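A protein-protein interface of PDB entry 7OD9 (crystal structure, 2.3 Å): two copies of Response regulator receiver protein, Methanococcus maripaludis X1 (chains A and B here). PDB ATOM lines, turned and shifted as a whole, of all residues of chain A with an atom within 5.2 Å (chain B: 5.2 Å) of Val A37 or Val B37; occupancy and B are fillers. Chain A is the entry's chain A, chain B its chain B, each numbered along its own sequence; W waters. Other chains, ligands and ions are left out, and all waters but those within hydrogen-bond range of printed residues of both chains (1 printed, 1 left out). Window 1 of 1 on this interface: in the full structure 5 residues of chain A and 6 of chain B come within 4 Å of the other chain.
OD1 of Asn A34 sits close to O of Val B38 (2.5 Å).
The side-chain amide nitrogen (ND2) of Asn B34 is in hydrogen-bond range of the backbone carbonyl oxygen (O) of Val A38 (2.5 Å).
The backbone NH (N) of Thr A13 lies within hydrogen-bond range of the backbone carbonyl oxygen (O) of Val A37, at 2.9 Å.
O of Val B11 is in hydrogen-bond range of N of Val B37 (3.1 Å).
N of Thr B13 is in hydrogen-bond range of O of Val B37 (2.8 Å).
The backbone carbonyl oxygen (O) of Val A11 is in hydrogen-bond range of the backbone NH (N) of Val A37 (3.2 Å).
Among the printed residues, pairs that only touch across the chains: Val A37 with Asn B34 (3.1 Å), Asn A34 with Val B37 (3.3 Å), Val A37 with Ile B10 (3.6 Å), Ile A10 with Ile B10 (3.7 Å), Ile A10 with Val B37 (3.8 Å), Ile A10 with Lys B12 (3.8 Å) and Val A37 with Val B37 (3.8 Å).
Val A37 touches just these residues of chain B: Ile B10 (3.6 Å), Asn B34 (3.1 Å) and Val B37 (3.8 Å).
Val B37 touches just these residues of chain A: Ile A10 (3.8 Å), Asn A34 (3.3 Å) and Val A37 (3.8 Å).
Printed residues of chain B within 4 Å of Asn A34: Val B37 (3.3 Å) and Val B38 (2.5 Å).
Printed residues of chain A within 4 Å of Val B38: Asn A34 (2.5 Å).
Printed residues of chain A within 4 Å of Lys B12: Ile A10.
Printed residues of chain A within 4 Å of Asn B34: Val A37 and Val A38.
Of the printed residues of chain B, Val A38 touches Asn B34 (2.5 Å).
Tyr A36 touches none of the printed residues of chain B.
The nearest residue of chain A that does not touch Val B37 is Lys A35 (5.0 Å).
Hydrophobic or aromatic side chains of chain B that line the printed part of chain A: Ile B10, Val B37 and Val B38.
Hydrophobic or aromatic side chains of chain A within 4 Å of the printed part of chain B: Ile A10, Val A37 and Val A38.
Among the printed residues, no Asp or Glu carboxylate lies within 4 Å of a Lys or Arg side-chain nitrogen of the other chain.
Ile A10 touches Val B37, and with the chains exchanged Val A37 touches Ile B10.
Asn A34 touches Val B37, and with the chains exchanged Val A37 touches Asn B34.
Asn A34 touches Val B38, and with the chains exchanged Val A38 touches Asn B34.
Val B37 touches its own counterpart, Val A37.
11 positions are printed for both chains.
Of the 9 pairs that touch across the chains among the printed residues, 8 have their exchanged pair printed and touching as well.
Water W1 lies within hydrogen-bond range of the side-chain amide oxygen of Asn B34 (3.0 Å) and the backbone carbonyl oxygen of Tyr A36 (3.0 Å).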
ATOM      1  N   SER A   9       1.113   2.247  22.233  1.00  0.00           N
ATOM      2  CA  SER A   9       2.116   3.305  22.280  1.00  0.00           C
ATOM      3  C   SER A   9       1.910   4.305  21.149  1.00  0.00           C
ATOM      4  O   SER A   9       2.017   3.959  19.972  1.00  0.00           O
ATOM      5  CB  SER A   9       3.526   2.714  22.209  1.00  0.00           C
ATOM      6  OG  SER A   9       4.510   3.727  22.323  1.00  0.00           O
ATOM      7  N   ILE A  10       1.611   5.549  21.515  1.00  0.00           N
ATOM      8  CA  ILE A  10       1.406   6.632  20.562  1.00  0.00           C
ATOM      9  C   ILE A  10       2.378   7.751  20.903  1.00  0.00           C
ATOM     10  O   ILE A  10       2.441   8.195  22.055  1.00  0.00           O
ATOM     11  CB  ILE A  10      -0.047   7.141  20.579  1.00  0.00           C
ATOM     12  CG1 ILE A  10      -1.012   6.004  20.241  1.00  0.00           C
ATOM     13  CG2 ILE A  10      -0.219   8.299  19.607  1.00  0.00           C
ATOM     14  CD1 ILE A  10      -2.468   6.418  20.236  1.00  0.00           C
ATOM     15  N   VAL A  11       3.129   8.202  19.906  1.00  0.00           N
ATOM     16  CA  VAL A  11       4.145   9.231  20.088  1.00  0.00           C
ATOM     17  C   VAL A  11       3.683  10.463  19.321  1.00  0.00           C
ATOM     18  O   VAL A  11       3.768  10.511  18.088  1.00  0.00           O
ATOM     19  CB  VAL A  11       5.526   8.762  19.616  1.00  0.00           C
ATOM     20  CG1 VAL A  11       6.558   9.862  19.818  1.00  0.00           C
ATOM     21  CG2 VAL A  11       5.935   7.494  20.347  1.00  0.00           C
ATOM     22  N   LYS A  12       3.184  11.462  20.048  1.00  0.00           N
ATOM     23  CA  LYS A  12       2.898  12.757  19.444  1.00  0.00           C
ATOM     24  C   LYS A  12       4.202  13.350  18.927  1.00  0.00           C
ATOM     25  O   LYS A  12       5.102  13.665  19.714  1.00  0.00           O
ATOM     26  CB  LYS A  12       2.225  13.691  20.451  1.00  0.00           C
ATOM     27  CG  LYS A  12       1.019  13.080  21.148  1.00  0.00           C
ATOM     28  CD  LYS A  12       0.144  14.144  21.790  1.00  0.00           C
ATOM     29  CE  LYS A  12       0.444  14.282  23.274  1.00  0.00           C
ATOM     30  NZ  LYS A  12      -0.785  14.159  24.107  1.00  0.00           N
ATOM     31  N   THR A  13       4.319  13.490  17.610  1.00  0.00           N
ATOM     32  CA  THR A  13       5.585  13.808  16.966  1.00  0.00           C
ATOM     33  C   THR A  13       5.489  15.145  16.243  1.00  0.00           C
ATOM     34  O   THR A  13       4.466  15.463  15.631  1.00  0.00           O
ATOM     35  CB  THR A  13       5.988  12.695  15.989  1.00  0.00           C
ATOM     36  OG1 THR A  13       6.364  11.527  16.730  1.00  0.00           O
ATOM     37  CG2 THR A  13       7.161  13.125  15.122  1.00  0.00           C
ATOM     38  N   ASN A  34       2.457   2.549  13.202  1.00  0.00           N
ATOM     39  CA  ASN A  34       1.260   2.659  14.016  1.00  0.00           C
ATOM     40  C   ASN A  34       1.530   3.370  15.332  1.00  0.00           C
ATOM     41  O   ASN A  34       0.797   3.164  16.307  1.00  0.00           O
ATOM     42  CB  ASN A  34       0.673   1.273  14.266  1.00  0.00           C
ATOM     43  CG  ASN A  34      -0.822   1.300  14.387  1.00  0.00           C
ATOM     44  OD1 ASN A  34      -1.390   0.631  15.235  1.00  0.00           O
ATOM     45  ND2 ASN A  34      -1.471   2.090  13.544  1.00  0.00           N
ATOM     46  N   LYS A  35       2.569   4.198  15.376  1.00  0.00           N
ATOM     47  CA  LYS A  35       3.005   4.892  16.579  1.00  0.00           C
ATOM     48  C   LYS A  35       3.014   6.400  16.409  1.00  0.00           C
ATOM     49  O   LYS A  35       2.400   7.119  17.207  1.00  0.00           O
ATOM     50  CB  LYS A  35       4.420   4.438  16.969  1.00  0.00           C
ATOM     51  CG  LYS A  35       4.579   2.979  17.324  1.00  0.00           C
ATOM     52  CD  LYS A  35       6.019   2.735  17.739  1.00  0.00           C
ATOM     53  CE  LYS A  35       6.336   3.491  19.019  1.00  0.00           C
ATOM     54  NZ  LYS A  35       7.733   3.269  19.478  1.00  0.00           N
ATOM     55  N   TYR A  36       3.702   6.898  15.387  1.00  0.00           N
ATOM     56  CA  TYR A  36       4.087   8.298  15.315  1.00  0.00           C
ATOM     57  C   TYR A  36       3.028   9.095  14.567  1.00  0.00           C
ATOM     58  O   TYR A  36       2.785   8.866  13.377  1.00  0.00           O
ATOM     59  CB  TYR A  36       5.458   8.426  14.655  1.00  0.00           C
ATOM     60  CG  TYR A  36       6.516   7.718  15.463  1.00  0.00           C
ATOM     61  CD1 TYR A  36       7.133   8.347  16.532  1.00  0.00           C
ATOM     62  CD2 TYR A  36       6.861   6.400  15.188  1.00  0.00           C
ATOM     63  CE1 TYR A  36       8.084   7.696  17.290  1.00  0.00           C
ATOM     64  CE2 TYR A  36       7.811   5.741  15.940  1.00  0.00           C
ATOM     65  CZ  TYR A  36       8.419   6.394  16.989  1.00  0.00           C
ATOM     66  OH  TYR A  36       9.366   5.743  17.742  1.00  0.00           O
ATOM     67  N   VAL A  37       2.399  10.019  15.280  1.00  0.00           N
ATOM     68  CA  VAL A  37       1.396  10.919  14.733  1.00  0.00           C
ATOM     69  C   VAL A  37       2.048  12.288  14.617  1.00  0.00           C
ATOM     70  O   VAL A  37       2.274  12.962  15.628  1.00  0.00           O
ATOM     71  CB  VAL A  37       0.144  10.972  15.616  1.00  0.00           C
ATOM     72  CG1 VAL A  37      -0.809  12.039  15.120  1.00  0.00           C
ATOM     73  CG2 VAL A  37      -0.536   9.609  15.657  1.00  0.00           C
ATOM     74  N   VAL A  38       2.374  12.698  13.393  1.00  0.00           N
ATOM     75  CA  VAL A  38       2.926  14.035  13.200  1.00  0.00           C
ATOM     76  C   VAL A  38       1.809  15.044  13.454  1.00  0.00           C
ATOM     77  O   VAL A  38       0.838  15.128  12.697  1.00  0.00           O
ATOM     78  CB  VAL A  38       3.550  14.205  11.808  1.00  0.00           C
ATOM     79  CG1 VAL A  38       2.634  13.676  10.716  1.00  0.00           C
ATOM     80  CG2 VAL A  38       3.904  15.667  11.561  1.00  0.00           C
ATOM     81  N   ILE A  39       1.929  15.791  14.554  1.00  0.00           N
ATOM     82  CA  ILE A  39       0.901  16.744  14.958  1.00  0.00           C
ATOM     83  C   ILE A  39       1.273  18.183  14.635  1.00  0.00           C
ATOM     84  O   ILE A  39       0.445  19.084  14.844  1.00  0.00           O
ATOM     85  CB  ILE A  39       0.587  16.618  16.465  1.00  0.00           C
ATOM     86  CG1 ILE A  39       1.787  17.074  17.295  1.00  0.00           C
ATOM     87  CG2 ILE A  39       0.208  15.188  16.813  1.00  0.00           C
ATOM     88  CD1 ILE A  39       1.579  16.951  18.788  1.00  0.00           C
ATOM     89  N   SER B   9      -7.549  14.670  17.054  1.00  0.00           N
ATOM     90  CA  SER B   9      -6.337  14.587  16.245  1.00  0.00           C
ATOM     91  C   SER B   9      -5.713  13.199  16.293  1.00  0.00           C
ATOM     92  O   SER B   9      -4.950  12.843  15.387  1.00  0.00           O
ATOM     93  CB  SER B   9      -5.323  15.638  16.700  1.00  0.00           C
ATOM     94  OG  SER B   9      -4.949  15.440  18.052  1.00  0.00           O
ATOM     95  N   ILE B  10      -6.015  12.413  17.326  1.00  0.00           N
ATOM     96  CA  ILE B  10      -5.562  11.030  17.441  1.00  0.00           C
ATOM     97  C   ILE B  10      -6.741  10.200  17.928  1.00  0.00           C
ATOM     98  O   ILE B  10      -7.302  10.480  18.993  1.00  0.00           O
ATOM     99  CB  ILE B  10      -4.371  10.877  18.404  1.00  0.00           C
ATOM    100  CG1 ILE B  10      -3.144  11.615  17.867  1.00  0.00           C
ATOM    101  CG2 ILE B  10      -4.055   9.406  18.627  1.00  0.00           C
ATOM    102  CD1 ILE B  10      -2.013  11.725  18.866  1.00  0.00           C
ATOM    103  N   VAL B  11      -7.119   9.185  17.158  1.00  0.00           N
ATOM    104  CA  VAL B  11      -8.272   8.345  17.469  1.00  0.00           C
ATOM    105  C   VAL B  11      -7.753   6.932  17.708  1.00  0.00           C
ATOM    106  O   VAL B  11      -7.407   6.217  16.760  1.00  0.00           O
ATOM    107  CB  VAL B  11      -9.326   8.368  16.357  1.00  0.00           C
ATOM    108  CG1 VAL B  11     -10.529   7.526  16.749  1.00  0.00           C
ATOM    109  CG2 VAL B  11      -9.747   9.798  16.053  1.00  0.00           C
ATOM    110  N   LYS B  12      -7.696   6.526  18.975  1.00  0.00           N
ATOM    111  CA  LYS B  12      -7.332   5.156  19.312  1.00  0.00           C
ATOM    112  C   LYS B  12      -8.399   4.207  18.783  1.00  0.00           C
ATOM    113  O   LYS B  12      -9.555   4.258  19.216  1.00  0.00           O
ATOM    114  CB  LYS B  12      -7.169   5.008  20.823  1.00  0.00           C
ATOM    115  CG  LYS B  12      -6.056   5.868  21.403  1.00  0.00           C
ATOM    116  CD  LYS B  12      -5.755   5.496  22.845  1.00  0.00           C
ATOM    117  CE  LYS B  12      -7.006   5.547  23.705  1.00  0.00           C
ATOM    118  NZ  LYS B  12      -7.388   6.946  24.043  1.00  0.00           N
ATOM    119  N   THR B  13      -8.016   3.349  17.842  1.00  0.00           N
ATOM    120  CA  THR B  13      -8.958   2.517  17.110  1.00  0.00           C
ATOM    121  C   THR B  13      -8.695   1.044  17.389  1.00  0.00           C
ATOM    122  O   THR B  13      -7.544   0.623  17.548  1.00  0.00           O
ATOM    123  CB  THR B  13      -8.872   2.789  15.603  1.00  0.00           C
ATOM    124  OG1 THR B  13      -8.913   4.203  15.374  1.00  0.00           O
ATOM    125  CG2 THR B  13     -10.034   2.135  14.871  1.00  0.00           C
ATOM    126  N   ASN B  34      -3.420  10.208   9.493  1.00  0.00           N
ATOM    127  CA  ASN B  34      -2.578  10.734  10.556  1.00  0.00           C
ATOM    128  C   ASN B  34      -3.273  10.747  11.910  1.00  0.00           C
ATOM    129  O   ASN B  34      -2.748  11.342  12.854  1.00  0.00           O
ATOM    130  CB  ASN B  34      -2.113  12.150  10.205  1.00  0.00           C
ATOM    131  CG  ASN B  34      -0.759  12.478  10.796  1.00  0.00           C
ATOM    132  OD1 ASN B  34       0.049  11.589  11.061  1.00  0.00           O
ATOM    133  ND2 ASN B  34      -0.512  13.762  11.020  1.00  0.00           N
ATOM    134  N   LYS B  35      -4.428  10.115  12.032  1.00  0.00           N
ATOM    135  CA  LYS B  35      -5.138  10.165  13.306  1.00  0.00           C
ATOM    136  C   LYS B  35      -5.520   8.794  13.840  1.00  0.00           C
ATOM    137  O   LYS B  35      -5.479   8.585  15.055  1.00  0.00           O
ATOM    138  CB  LYS B  35      -6.399  11.040  13.174  1.00  0.00           C
ATOM    139  CG  LYS B  35      -7.395  10.556  12.137  1.00  0.00           C
ATOM    140  CD  LYS B  35      -8.256  11.695  11.625  1.00  0.00           C
ATOM    141  CE  LYS B  35      -9.243  12.159  12.682  1.00  0.00           C
ATOM    142  NZ  LYS B  35     -10.281  13.062  12.113  1.00  0.00           N
ATOM    143  N   TYR B  36      -5.883   7.854  12.970  1.00  0.00           N
ATOM    144  CA  TYR B  36      -6.392   6.560  13.413  1.00  0.00           C
ATOM    145  C   TYR B  36      -5.221   5.631  13.705  1.00  0.00           C
ATOM    146  O   TYR B  36      -4.478   5.245  12.796  1.00  0.00           O
ATOM    147  CB  TYR B  36      -7.334   5.979  12.364  1.00  0.00           C
ATOM    148  CG  TYR B  36      -8.574   6.822  12.184  1.00  0.00           C
ATOM    149  CD1 TYR B  36      -9.528   6.902  13.189  1.00  0.00           C
ATOM    150  CD2 TYR B  36      -8.778   7.558  11.026  1.00  0.00           C
ATOM    151  CE1 TYR B  36     -10.657   7.681  13.042  1.00  0.00           C
ATOM    152  CE2 TYR B  36      -9.907   8.341  10.868  1.00  0.00           C
ATOM    153  CZ  TYR B  36     -10.843   8.398  11.880  1.00  0.00           C
ATOM    154  OH  TYR B  36     -11.968   9.175  11.731  1.00  0.00           O
ATOM    155  N   VAL B  37      -5.058   5.278  14.976  1.00  0.00           N
ATOM    156  CA  VAL B  37      -3.981   4.413  15.439  1.00  0.00           C
ATOM    157  C   VAL B  37      -4.619   3.126  15.945  1.00  0.00           C
ATOM    158  O   VAL B  37      -5.323   3.130  16.963  1.00  0.00           O
ATOM    159  CB  VAL B  37      -3.139   5.088  16.531  1.00  0.00           C
ATOM    160  CG1 VAL B  37      -2.258   4.068  17.238  1.00  0.00           C
ATOM    161  CG2 VAL B  37      -2.301   6.212  15.938  1.00  0.00           C
ATOM    162  N   VAL B  38      -4.385   2.026  15.232  1.00  0.00           N
ATOM    163  CA  VAL B  38      -4.963   0.735  15.597  1.00  0.00           C
ATOM    164  C   VAL B  38      -4.280   0.242  16.869  1.00  0.00           C
ATOM    165  O   VAL B  38      -3.152  -0.252  16.826  1.00  0.00           O
ATOM    166  CB  VAL B  38      -4.819  -0.285  14.462  1.00  0.00           C
ATOM    167  CG1 VAL B  38      -5.434  -1.617  14.866  1.00  0.00           C
ATOM    168  CG2 VAL B  38      -5.465   0.242  13.190  1.00  0.00           C
ATOM    169  N   ILE B  39      -4.962   0.355  18.008  1.00  0.00           N
ATOM    170  CA  ILE B  39      -4.360  -0.028  19.280  1.00  0.00           C
ATOM    171  C   ILE B  39      -4.711  -1.449  19.695  1.00  0.00           C
ATOM    172  O   ILE B  39      -4.312  -1.879  20.785  1.00  0.00           O
ATOM    173  CB  ILE B  39      -4.743   0.962  20.395  1.00  0.00           C
ATOM    174  CG1 ILE B  39      -6.221   0.812  20.752  1.00  0.00           C
ATOM    175  CG2 ILE B  39      -4.424   2.388  19.970  1.00  0.00           C
ATOM    176  CD1 ILE B  39      -6.544   1.218  22.168  1.00  0.00           C
HETATM  177  O   HOH W   1       2.336   9.761  10.514  1.00  0.00           O
